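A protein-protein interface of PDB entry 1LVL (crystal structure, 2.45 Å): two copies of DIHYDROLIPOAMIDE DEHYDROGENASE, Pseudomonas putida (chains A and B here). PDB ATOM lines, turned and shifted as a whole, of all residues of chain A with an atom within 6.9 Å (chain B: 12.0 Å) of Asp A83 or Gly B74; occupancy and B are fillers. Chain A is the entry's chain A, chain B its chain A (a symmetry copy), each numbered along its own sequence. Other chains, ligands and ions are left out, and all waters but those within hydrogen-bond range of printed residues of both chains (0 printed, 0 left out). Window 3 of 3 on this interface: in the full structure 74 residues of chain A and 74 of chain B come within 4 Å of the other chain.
Leu A82 touches just one residue of chain B: Gly B74. No residue of chain B comes within 4 Å of Gly A85. Of the printed residues of chain B, Gln A86 touches Pro B72 (3.1 Å) and Gly B74 (3.5 Å). Of the printed residues of chain A, Pro B72 touches Gln A86 and Trp A90. Printed residues of chain A within 4 Å of Ile B75: Val A57, Phe A61 and Arg A81. The nearest residue of chain B that does not touch Asp A83 is Leu B73 (4.8 Å). The nearest residue of chain A that does not touch Gly B74 is Ser A87 (4.5 Å).
Hydrophobic or aromatic side chains of chain B that line the printed part of chain A: Pro B72, Leu B73 and Ile B75. Hydrophobic or aromatic side chains of chain A that line the printed part of chain B: Val A57, Phe A61 and Trp A90. Among the printed residues, no Asp or Glu carboxylate lies within 4 Å of a Lys or Arg side-chain nitrogen of the other chain.
Among the printed residues, pairs that only touch across the chains: Val A57 with Leu B73 (3.9 Å), Val A57 with Ile B75 (3.6 Å), Phe A61 with Ile B75 (3.3 Å), Arg A81 with Gly B74 (3.7 Å), Arg A81 with Ile B75 (3.1 Å), Leu A82 with Gly B74 (3.8 Å), Asp A83 with Gly B74 (3.7 Å), Gln A86 with Gly B74 (3.5 Å), Trp A90 with Pro B72 (3.2 Å), Trp A90 with Leu B73 (3.6 Å) and Trp A90 with Ser B381 (3.2 Å).
OG of Ser A87 sits at hydrogen-bond distance from O of Leu B73 (2.8 Å). The backbone carbonyl oxygen of Gln A86 lies close to the backbone carbonyl oxygen of Pro B72 (3.1 Å). The backbone carbonyl oxygen (O) of Ser B76 lies within hydrogen-bond range of the backbone NH (N) of Arg A81 (2.7 Å).
The guanidinium group of Arg A81 lies within salt-bridge range of the side-chain carboxylate of Asp A83 (2.8 Å).
No position is printed for both chains.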
ATOM      1  N   VAL A  57     -18.450  22.345  -7.340  1.00  0.00           N
ATOM      2  CA  VAL A  57     -17.092  22.308  -6.816  1.00  0.00           C
ATOM      3  C   VAL A  57     -16.939  23.337  -5.719  1.00  0.00           C
ATOM      4  O   VAL A  57     -16.113  23.152  -4.817  1.00  0.00           O
ATOM      5  CB  VAL A  57     -16.045  22.510  -7.984  1.00  0.00           C
ATOM      6  CG1 VAL A  57     -16.470  23.604  -8.923  1.00  0.00           C
ATOM      7  CG2 VAL A  57     -14.688  22.955  -7.435  1.00  0.00           C
ATOM      8  N   PHE A  61     -15.601  22.394  -1.863  1.00  0.00           N
ATOM      9  CA  PHE A  61     -14.480  23.117  -1.263  1.00  0.00           C
ATOM     10  C   PHE A  61     -14.927  23.661   0.088  1.00  0.00           C
ATOM     11  O   PHE A  61     -14.213  23.563   1.092  1.00  0.00           O
ATOM     12  CB  PHE A  61     -14.010  24.303  -2.123  1.00  0.00           C
ATOM     13  CG  PHE A  61     -12.734  24.862  -1.501  1.00  0.00           C
ATOM     14  CD1 PHE A  61     -11.596  24.075  -1.472  1.00  0.00           C
ATOM     15  CD2 PHE A  61     -12.726  26.135  -0.959  1.00  0.00           C
ATOM     16  CE1 PHE A  61     -10.437  24.552  -0.906  1.00  0.00           C
ATOM     17  CE2 PHE A  61     -11.559  26.608  -0.393  1.00  0.00           C
ATOM     18  CZ  PHE A  61     -10.420  25.824  -0.365  1.00  0.00           C
ATOM     19  N   ARG A  81      -7.052  23.404  -0.095  1.00  0.00           N
ATOM     20  CA  ARG A  81      -6.491  24.227  -1.150  1.00  0.00           C
ATOM     21  C   ARG A  81      -7.351  24.027  -2.362  1.00  0.00           C
ATOM     22  O   ARG A  81      -7.916  22.943  -2.579  1.00  0.00           O
ATOM     23  CB  ARG A  81      -5.136  23.790  -1.493  1.00  0.00           C
ATOM     24  CG  ARG A  81      -4.150  24.126  -0.418  1.00  0.00           C
ATOM     25  CD  ARG A  81      -2.813  23.541  -0.813  1.00  0.00           C
ATOM     26  NE  ARG A  81      -2.511  23.751  -2.232  1.00  0.00           N
ATOM     27  CZ  ARG A  81      -2.268  24.946  -2.818  1.00  0.00           C
ATOM     28  NH1 ARG A  81      -2.272  26.105  -2.150  1.00  0.00           N
ATOM     29  NH2 ARG A  81      -2.040  24.981  -4.129  1.00  0.00           N
ATOM     30  N   LEU A  82      -7.461  25.122  -3.115  1.00  0.00           N
ATOM     31  CA  LEU A  82      -8.234  25.188  -4.349  1.00  0.00           C
ATOM     32  C   LEU A  82      -7.455  26.079  -5.279  1.00  0.00           C
ATOM     33  O   LEU A  82      -7.152  27.245  -4.998  1.00  0.00           O
ATOM     34  CB  LEU A  82      -9.588  25.846  -4.194  1.00  0.00           C
ATOM     35  CG  LEU A  82     -10.376  26.042  -5.454  1.00  0.00           C
ATOM     36  CD1 LEU A  82     -11.644  25.213  -5.486  1.00  0.00           C
ATOM     37  CD2 LEU A  82     -10.812  27.458  -5.476  1.00  0.00           C
ATOM     38  N   ASP A  83      -7.090  25.454  -6.378  1.00  0.00           N
ATOM     39  CA  ASP A  83      -6.448  26.139  -7.464  1.00  0.00           C
ATOM     40  C   ASP A  83      -7.449  25.746  -8.555  1.00  0.00           C
ATOM     41  O   ASP A  83      -7.646  24.565  -8.887  1.00  0.00           O
ATOM     42  CB  ASP A  83      -5.026  25.552  -7.524  1.00  0.00           C
ATOM     43  CG  ASP A  83      -4.124  25.988  -6.335  1.00  0.00           C
ATOM     44  OD1 ASP A  83      -4.469  25.749  -5.171  1.00  0.00           O
ATOM     45  OD2 ASP A  83      -3.055  26.565  -6.571  1.00  0.00           O
ATOM     46  N   ILE A  84      -8.188  26.809  -8.941  1.00  0.00           N
ATOM     47  CA  ILE A  84      -9.383  26.731  -9.787  1.00  0.00           C
ATOM     48  C   ILE A  84      -9.152  26.369 -11.236  1.00  0.00           C
ATOM     49  O   ILE A  84     -10.114  26.112 -11.983  1.00  0.00           O
ATOM     50  CB  ILE A  84     -10.287  28.040  -9.894  1.00  0.00           C
ATOM     51  CG1 ILE A  84      -9.577  29.236  -9.401  1.00  0.00           C
ATOM     52  CG2 ILE A  84     -11.606  27.819  -9.180  1.00  0.00           C
ATOM     53  CD1 ILE A  84      -8.448  29.613 -10.358  1.00  0.00           C
ATOM     54  N   GLY A  85      -7.898  26.342 -11.650  1.00  0.00           N
ATOM     55  CA  GLY A  85      -7.596  25.898 -12.993  1.00  0.00           C
ATOM     56  C   GLY A  85      -8.238  24.542 -13.278  1.00  0.00           C
ATOM     57  O   GLY A  85      -9.013  24.360 -14.230  1.00  0.00           O
ATOM     58  N   GLN A  86      -7.966  23.602 -12.360  1.00  0.00           N
ATOM     59  CA  GLN A  86      -8.501  22.251 -12.429  1.00  0.00           C
ATOM     60  C   GLN A  86     -10.008  22.225 -12.292  1.00  0.00           C
ATOM     61  O   GLN A  86     -10.657  21.513 -13.050  1.00  0.00           O
ATOM     62  CB  GLN A  86      -7.836  21.446 -11.358  1.00  0.00           C
ATOM     63  CG  GLN A  86      -6.511  20.873 -11.792  1.00  0.00           C
ATOM     64  CD  GLN A  86      -6.690  19.510 -12.430  1.00  0.00           C
ATOM     65  OE1 GLN A  86      -7.703  19.192 -13.049  1.00  0.00           O
ATOM     66  NE2 GLN A  86      -5.702  18.644 -12.278  1.00  0.00           N
ATOM     67  N   SER A  87     -10.626  23.063 -11.464  1.00  0.00           N
ATOM     68  CA  SER A  87     -12.076  23.113 -11.315  1.00  0.00           C
ATOM     69  C   SER A  87     -12.689  23.482 -12.655  1.00  0.00           C
ATOM     70  O   SER A  87     -13.678  22.906 -13.140  1.00  0.00           O
ATOM     71  CB  SER A  87     -12.413  24.161 -10.265  1.00  0.00           C
ATOM     72  OG  SER A  87     -11.440  24.122  -9.217  1.00  0.00           O
ATOM     73  N   VAL A  88     -12.038  24.437 -13.306  1.00  0.00           N
ATOM     74  CA  VAL A  88     -12.499  24.839 -14.614  1.00  0.00           C
ATOM     75  C   VAL A  88     -12.207  23.792 -15.696  1.00  0.00           C
ATOM     76  O   VAL A  88     -13.134  23.473 -16.455  1.00  0.00           O
ATOM     77  CB  VAL A  88     -11.872  26.188 -14.924  1.00  0.00           C
ATOM     78  CG1 VAL A  88     -12.363  26.643 -16.296  1.00  0.00           C
ATOM     79  CG2 VAL A  88     -12.294  27.221 -13.850  1.00  0.00           C
ATOM     80  N   TRP A  90     -12.202  20.718 -15.295  1.00  0.00           N
ATOM     81  CA  TRP A  90     -13.249  19.727 -15.027  1.00  0.00           C
ATOM     82  C   TRP A  90     -14.577  20.106 -15.680  1.00  0.00           C
ATOM     83  O   TRP A  90     -15.253  19.306 -16.354  1.00  0.00           O
ATOM     84  CB  TRP A  90     -13.417  19.558 -13.456  1.00  0.00           C
ATOM     85  CG  TRP A  90     -14.601  18.690 -12.987  1.00  0.00           C
ATOM     86  CD1 TRP A  90     -14.580  17.351 -13.246  1.00  0.00           C
ATOM     87  CD2 TRP A  90     -15.821  19.089 -12.449  1.00  0.00           C
ATOM     88  NE1 TRP A  90     -15.773  16.913 -12.924  1.00  0.00           N
ATOM     89  CE2 TRP A  90     -16.540  17.894 -12.449  1.00  0.00           C
ATOM     90  CE3 TRP A  90     -16.438  20.231 -11.987  1.00  0.00           C
ATOM     91  CZ2 TRP A  90     -17.849  17.785 -12.015  1.00  0.00           C
ATOM     92  CZ3 TRP A  90     -17.748  20.133 -11.552  1.00  0.00           C
ATOM     93  CH2 TRP A  90     -18.446  18.937 -11.564  1.00  0.00           C
ATOM     94  N   LYS A 168      -9.046  32.056 -14.056  1.00  0.00           N
ATOM     95  CA  LYS A 168      -7.744  31.454 -13.990  1.00  0.00           C
ATOM     96  C   LYS A 168      -7.128  31.780 -12.637  1.00  0.00           C
ATOM     97  O   LYS A 168      -6.083  31.223 -12.245  1.00  0.00           O
ATOM     98  CB  LYS A 168      -6.853  31.967 -15.149  1.00  0.00           C
ATOM     99  CG  LYS A 168      -6.848  33.438 -15.566  1.00  0.00           C
ATOM    100  CD  LYS A 168      -5.830  33.700 -16.698  1.00  0.00           C
ATOM    101  CE  LYS A 168      -4.391  33.994 -16.231  1.00  0.00           C
ATOM    102  NZ  LYS A 168      -4.197  35.396 -15.880  1.00  0.00           N
ATOM    103  N   GLN B  63     -15.983  12.267   1.406  1.00  0.00           N
ATOM    104  CA  GLN B  63     -15.697  13.367   0.493  1.00  0.00           C
ATOM    105  C   GLN B  63     -14.499  14.175   0.952  1.00  0.00           C
ATOM    106  O   GLN B  63     -13.624  14.395   0.120  1.00  0.00           O
ATOM    107  CB  GLN B  63     -16.855  14.313   0.355  1.00  0.00           C
ATOM    108  CG  GLN B  63     -18.208  13.766  -0.066  1.00  0.00           C
ATOM    109  CD  GLN B  63     -18.299  12.790  -1.239  1.00  0.00           C
ATOM    110  OE1 GLN B  63     -17.532  11.839  -1.414  1.00  0.00           O
ATOM    111  NE2 GLN B  63     -19.341  12.883  -2.047  1.00  0.00           N
ATOM    112  N   ALA B  64     -14.297  14.609   2.198  1.00  0.00           N
ATOM    113  CA  ALA B  64     -13.008  15.197   2.514  1.00  0.00           C
ATOM    114  C   ALA B  64     -11.910  14.140   2.502  1.00  0.00           C
ATOM    115  O   ALA B  64     -10.764  14.545   2.369  1.00  0.00           O
ATOM    116  CB  ALA B  64     -12.998  15.857   3.859  1.00  0.00           C
ATOM    117  N   SER B  65     -12.101  12.816   2.580  1.00  0.00           N
ATOM    118  CA  SER B  65     -10.995  11.858   2.413  1.00  0.00           C
ATOM    119  C   SER B  65     -10.480  11.734   0.993  1.00  0.00           C
ATOM    120  O   SER B  65      -9.266  11.709   0.763  1.00  0.00           O
ATOM    121  CB  SER B  65     -11.378  10.473   2.829  1.00  0.00           C
ATOM    122  OG  SER B  65     -11.525  10.604   4.225  1.00  0.00           O
ATOM    123  N   ARG B  66     -11.379  11.711   0.009  1.00  0.00           N
ATOM    124  CA  ARG B  66     -10.969  11.636  -1.375  1.00  0.00           C
ATOM    125  C   ARG B  66     -10.036  12.779  -1.772  1.00  0.00           C
ATOM    126  O   ARG B  66      -9.117  12.577  -2.572  1.00  0.00           O
ATOM    127  CB  ARG B  66     -12.200  11.627  -2.270  1.00  0.00           C
ATOM    128  CG  ARG B  66     -12.943  12.903  -2.535  1.00  0.00           C
ATOM    129  CD  ARG B  66     -13.875  12.694  -3.724  1.00  0.00           C
ATOM    130  NE  ARG B  66     -14.726  13.859  -3.886  1.00  0.00           N
ATOM    131  CZ  ARG B  66     -15.782  13.897  -4.711  1.00  0.00           C
ATOM    132  NH1 ARG B  66     -16.155  12.867  -5.484  1.00  0.00           N
ATOM    133  NH2 ARG B  66     -16.543  14.992  -4.686  1.00  0.00           N
ATOM    134  N   PHE B  67     -10.157  13.952  -1.151  1.00  0.00           N
ATOM    135  CA  PHE B  67      -9.271  15.046  -1.488  1.00  0.00           C
ATOM    136  C   PHE B  67      -7.846  14.953  -0.964  1.00  0.00           C
ATOM    137  O   PHE B  67      -7.127  15.970  -0.967  1.00  0.00           O
ATOM    138  CB  PHE B  67      -9.930  16.365  -1.048  1.00  0.00           C
ATOM    139  CG  PHE B  67     -11.202  16.630  -1.884  1.00  0.00           C
ATOM    140  CD1 PHE B  67     -11.264  16.294  -3.242  1.00  0.00           C
ATOM    141  CD2 PHE B  67     -12.340  17.161  -1.288  1.00  0.00           C
ATOM    142  CE1 PHE B  67     -12.438  16.480  -3.971  1.00  0.00           C
ATOM    143  CE2 PHE B  67     -13.507  17.337  -2.038  1.00  0.00           C
ATOM    144  CZ  PHE B  67     -13.571  17.001  -3.371  1.00  0.00           C
ATOM    145  N   THR B  68      -7.433  13.776  -0.467  1.00  0.00           N
ATOM    146  CA  THR B  68      -6.027  13.585  -0.152  1.00  0.00           C
ATOM    147  C   THR B  68      -5.344  13.072  -1.415  1.00  0.00           C
ATOM    148  O   THR B  68      -4.138  13.238  -1.623  1.00  0.00           O
ATOM    149  CB  THR B  68      -5.806  12.559   0.986  1.00  0.00           C
ATOM    150  OG1 THR B  68      -6.650  11.433   0.799  1.00  0.00           O
ATOM    151  CG2 THR B  68      -6.069  13.203   2.318  1.00  0.00           C
ATOM    152  N   GLU B  69      -6.126  12.386  -2.250  1.00  0.00           N
ATOM    153  CA  GLU B  69      -5.691  11.902  -3.540  1.00  0.00           C
ATOM    154  C   GLU B  69      -6.068  13.008  -4.533  1.00  0.00           C
ATOM    155  O   GLU B  69      -6.941  13.842  -4.256  1.00  0.00           O
ATOM    156  CB  GLU B  69      -6.422  10.616  -3.920  1.00  0.00           C
ATOM    157  CG  GLU B  69      -5.501   9.381  -3.996  1.00  0.00           C
ATOM    158  CD  GLU B  69      -5.416   8.630  -5.340  1.00  0.00           C
ATOM    159  OE1 GLU B  69      -6.454   8.343  -5.956  1.00  0.00           O
ATOM    160  OE2 GLU B  69      -4.290   8.322  -5.758  1.00  0.00           O
ATOM    161  N   PRO B  70      -5.436  13.103  -5.711  1.00  0.00           N
ATOM    162  CA  PRO B  70      -5.807  14.036  -6.762  1.00  0.00           C
ATOM    163  C   PRO B  70      -7.214  13.801  -7.223  1.00  0.00           C
ATOM    164  O   PRO B  70      -7.647  12.649  -7.374  1.00  0.00           O
ATOM    165  CB  PRO B  70      -4.799  13.798  -7.845  1.00  0.00           C
ATOM    166  CG  PRO B  70      -4.419  12.341  -7.643  1.00  0.00           C
ATOM    167  CD  PRO B  70      -4.270  12.317  -6.129  1.00  0.00           C
ATOM    168  N   SER B  71      -7.881  14.928  -7.437  1.00  0.00           N
ATOM    169  CA  SER B  71      -9.239  14.919  -7.936  1.00  0.00           C
ATOM    170  C   SER B  71      -9.256  15.821  -9.168  1.00  0.00           C
ATOM    171  O   SER B  71      -8.464  16.762  -9.225  1.00  0.00           O
ATOM    172  CB  SER B  71     -10.207  15.464  -6.876  1.00  0.00           C
ATOM    173  OG  SER B  71     -11.514  14.909  -7.088  1.00  0.00           O
ATOM    174  N   PRO B  72     -10.113  15.629 -10.179  1.00  0.00           N
ATOM    175  CA  PRO B  72     -10.338  16.619 -11.223  1.00  0.00           C
ATOM    176  C   PRO B  72     -10.982  17.895 -10.726  1.00  0.00           C
ATOM    177  O   PRO B  72     -11.065  18.851 -11.480  1.00  0.00           O
ATOM    178  CB  PRO B  72     -11.172  15.906 -12.275  1.00  0.00           C
ATOM    179  CG  PRO B  72     -11.780  14.734 -11.557  1.00  0.00           C
ATOM    180  CD  PRO B  72     -10.701  14.345 -10.559  1.00  0.00           C
ATOM    181  N   LEU B  73     -11.468  17.973  -9.483  1.00  0.00           N
ATOM    182  CA  LEU B  73     -12.062  19.204  -8.997  1.00  0.00           C
ATOM    183  C   LEU B  73     -11.001  20.210  -8.542  1.00  0.00           C
ATOM    184  O   LEU B  73     -11.285  21.397  -8.400  1.00  0.00           O
ATOM    185  CB  LEU B  73     -13.069  18.812  -7.888  1.00  0.00           C
ATOM    186  CG  LEU B  73     -14.528  18.602  -8.372  1.00  0.00           C
ATOM    187  CD1 LEU B  73     -14.585  17.531  -9.456  1.00  0.00           C
ATOM    188  CD2 LEU B  73     -15.413  18.207  -7.191  1.00  0.00           C
ATOM    189  N   GLY B  74      -9.744  19.838  -8.374  1.00  0.00           N
ATOM    190  CA  GLY B  74      -8.683  20.759  -7.983  1.00  0.00           C
ATOM    191  C   GLY B  74      -8.637  21.061  -6.502  1.00  0.00           C
ATOM    192  O   GLY B  74      -7.779  21.842  -6.104  1.00  0.00           O
ATOM    193  N   ILE B  75      -9.480  20.480  -5.639  1.00  0.00           N
ATOM    194  CA  ILE B  75      -9.459  20.717  -4.178  1.00  0.00           C
ATOM    195  C   ILE B  75      -8.470  19.730  -3.539  1.00  0.00           C
ATOM    196  O   ILE B  75      -8.429  18.544  -3.951  1.00  0.00           O
ATOM    197  CB  ILE B  75     -10.855  20.474  -3.542  1.00  0.00           C
ATOM    198  CG1 ILE B  75     -11.919  21.238  -4.303  1.00  0.00           C
ATOM    199  CG2 ILE B  75     -10.809  20.875  -2.062  1.00  0.00           C
ATOM    200  CD1 ILE B  75     -13.391  20.920  -4.026  1.00  0.00           C
ATOM    201  N   SER B  76      -7.720  20.177  -2.524  1.00  0.00           N
ATOM    202  CA  SER B  76      -6.775  19.323  -1.808  1.00  0.00           C
ATOM    203  C   SER B  76      -6.823  19.584  -0.285  1.00  0.00           C
ATOM    204  O   SER B  76      -6.901  20.750   0.139  1.00  0.00           O
ATOM    205  CB  SER B  76      -5.377  19.602  -2.383  1.00  0.00           C
ATOM    206  OG  SER B  76      -4.339  18.705  -1.985  1.00  0.00           O
ATOM    207  N   VAL B  77      -6.837  18.569   0.593  1.00  0.00           N
ATOM    208  CA  VAL B  77      -6.803  18.799   2.029  1.00  0.00           C
ATOM    209  C   VAL B  77      -5.826  17.769   2.579  1.00  0.00           C
ATOM    210  O   VAL B  77      -5.572  16.721   1.981  1.00  0.00           O
ATOM    211  CB  VAL B  77      -8.198  18.600   2.725  1.00  0.00           C
ATOM    212  CG1 VAL B  77      -9.292  19.376   2.053  1.00  0.00           C
ATOM    213  CG2 VAL B  77      -8.693  17.202   2.558  1.00  0.00           C
ATOM    214  N   ALA B  78      -5.176  18.062   3.675  1.00  0.00           N
ATOM    215  CA  ALA B  78      -4.353  17.101   4.383  1.00  0.00           C
ATOM    216  C   ALA B  78      -5.054  16.684   5.685  1.00  0.00           C
ATOM    217  O   ALA B  78      -5.974  17.356   6.166  1.00  0.00           O
ATOM    218  CB  ALA B  78      -3.017  17.727   4.737  1.00  0.00           C
ATOM    219  N   SER B 381     -23.059  17.343 -13.267  1.00  0.00           N
ATOM    220  CA  SER B 381     -22.584  18.346 -12.318  1.00  0.00           C
ATOM    221  C   SER B 381     -22.218  17.733 -10.990  1.00  0.00           C
ATOM    222  O   SER B 381     -21.270  18.140 -10.347  1.00  0.00           O
ATOM    223  CB  SER B 381     -23.614  19.440 -12.060  1.00  0.00           C
ATOM    224  OG  SER B 381     -25.003  19.195 -11.808  1.00  0.00           O
ATOM    225  N   GLU B 383     -20.977  14.612 -10.227  1.00  0.00           N
ATOM    226  CA  GLU B 383     -20.071  13.469 -10.358  1.00  0.00           C
ATOM    227  C   GLU B 383     -20.789  12.128 -10.491  1.00  0.00           C
ATOM    228  O   GLU B 383     -20.341  11.052 -10.132  1.00  0.00           O
ATOM    229  CB  GLU B 383     -19.118  13.449  -9.184  1.00  0.00           C
ATOM    230  CG  GLU B 383     -18.197  14.632  -9.311  1.00  0.00           C
ATOM    231  CD  GLU B 383     -17.203  14.710  -8.183  1.00  0.00           C
ATOM    232  OE1 GLU B 383     -16.171  14.039  -8.251  1.00  0.00           O
ATOM    233  OE2 GLU B 383     -17.474  15.457  -7.249  1.00  0.00           O
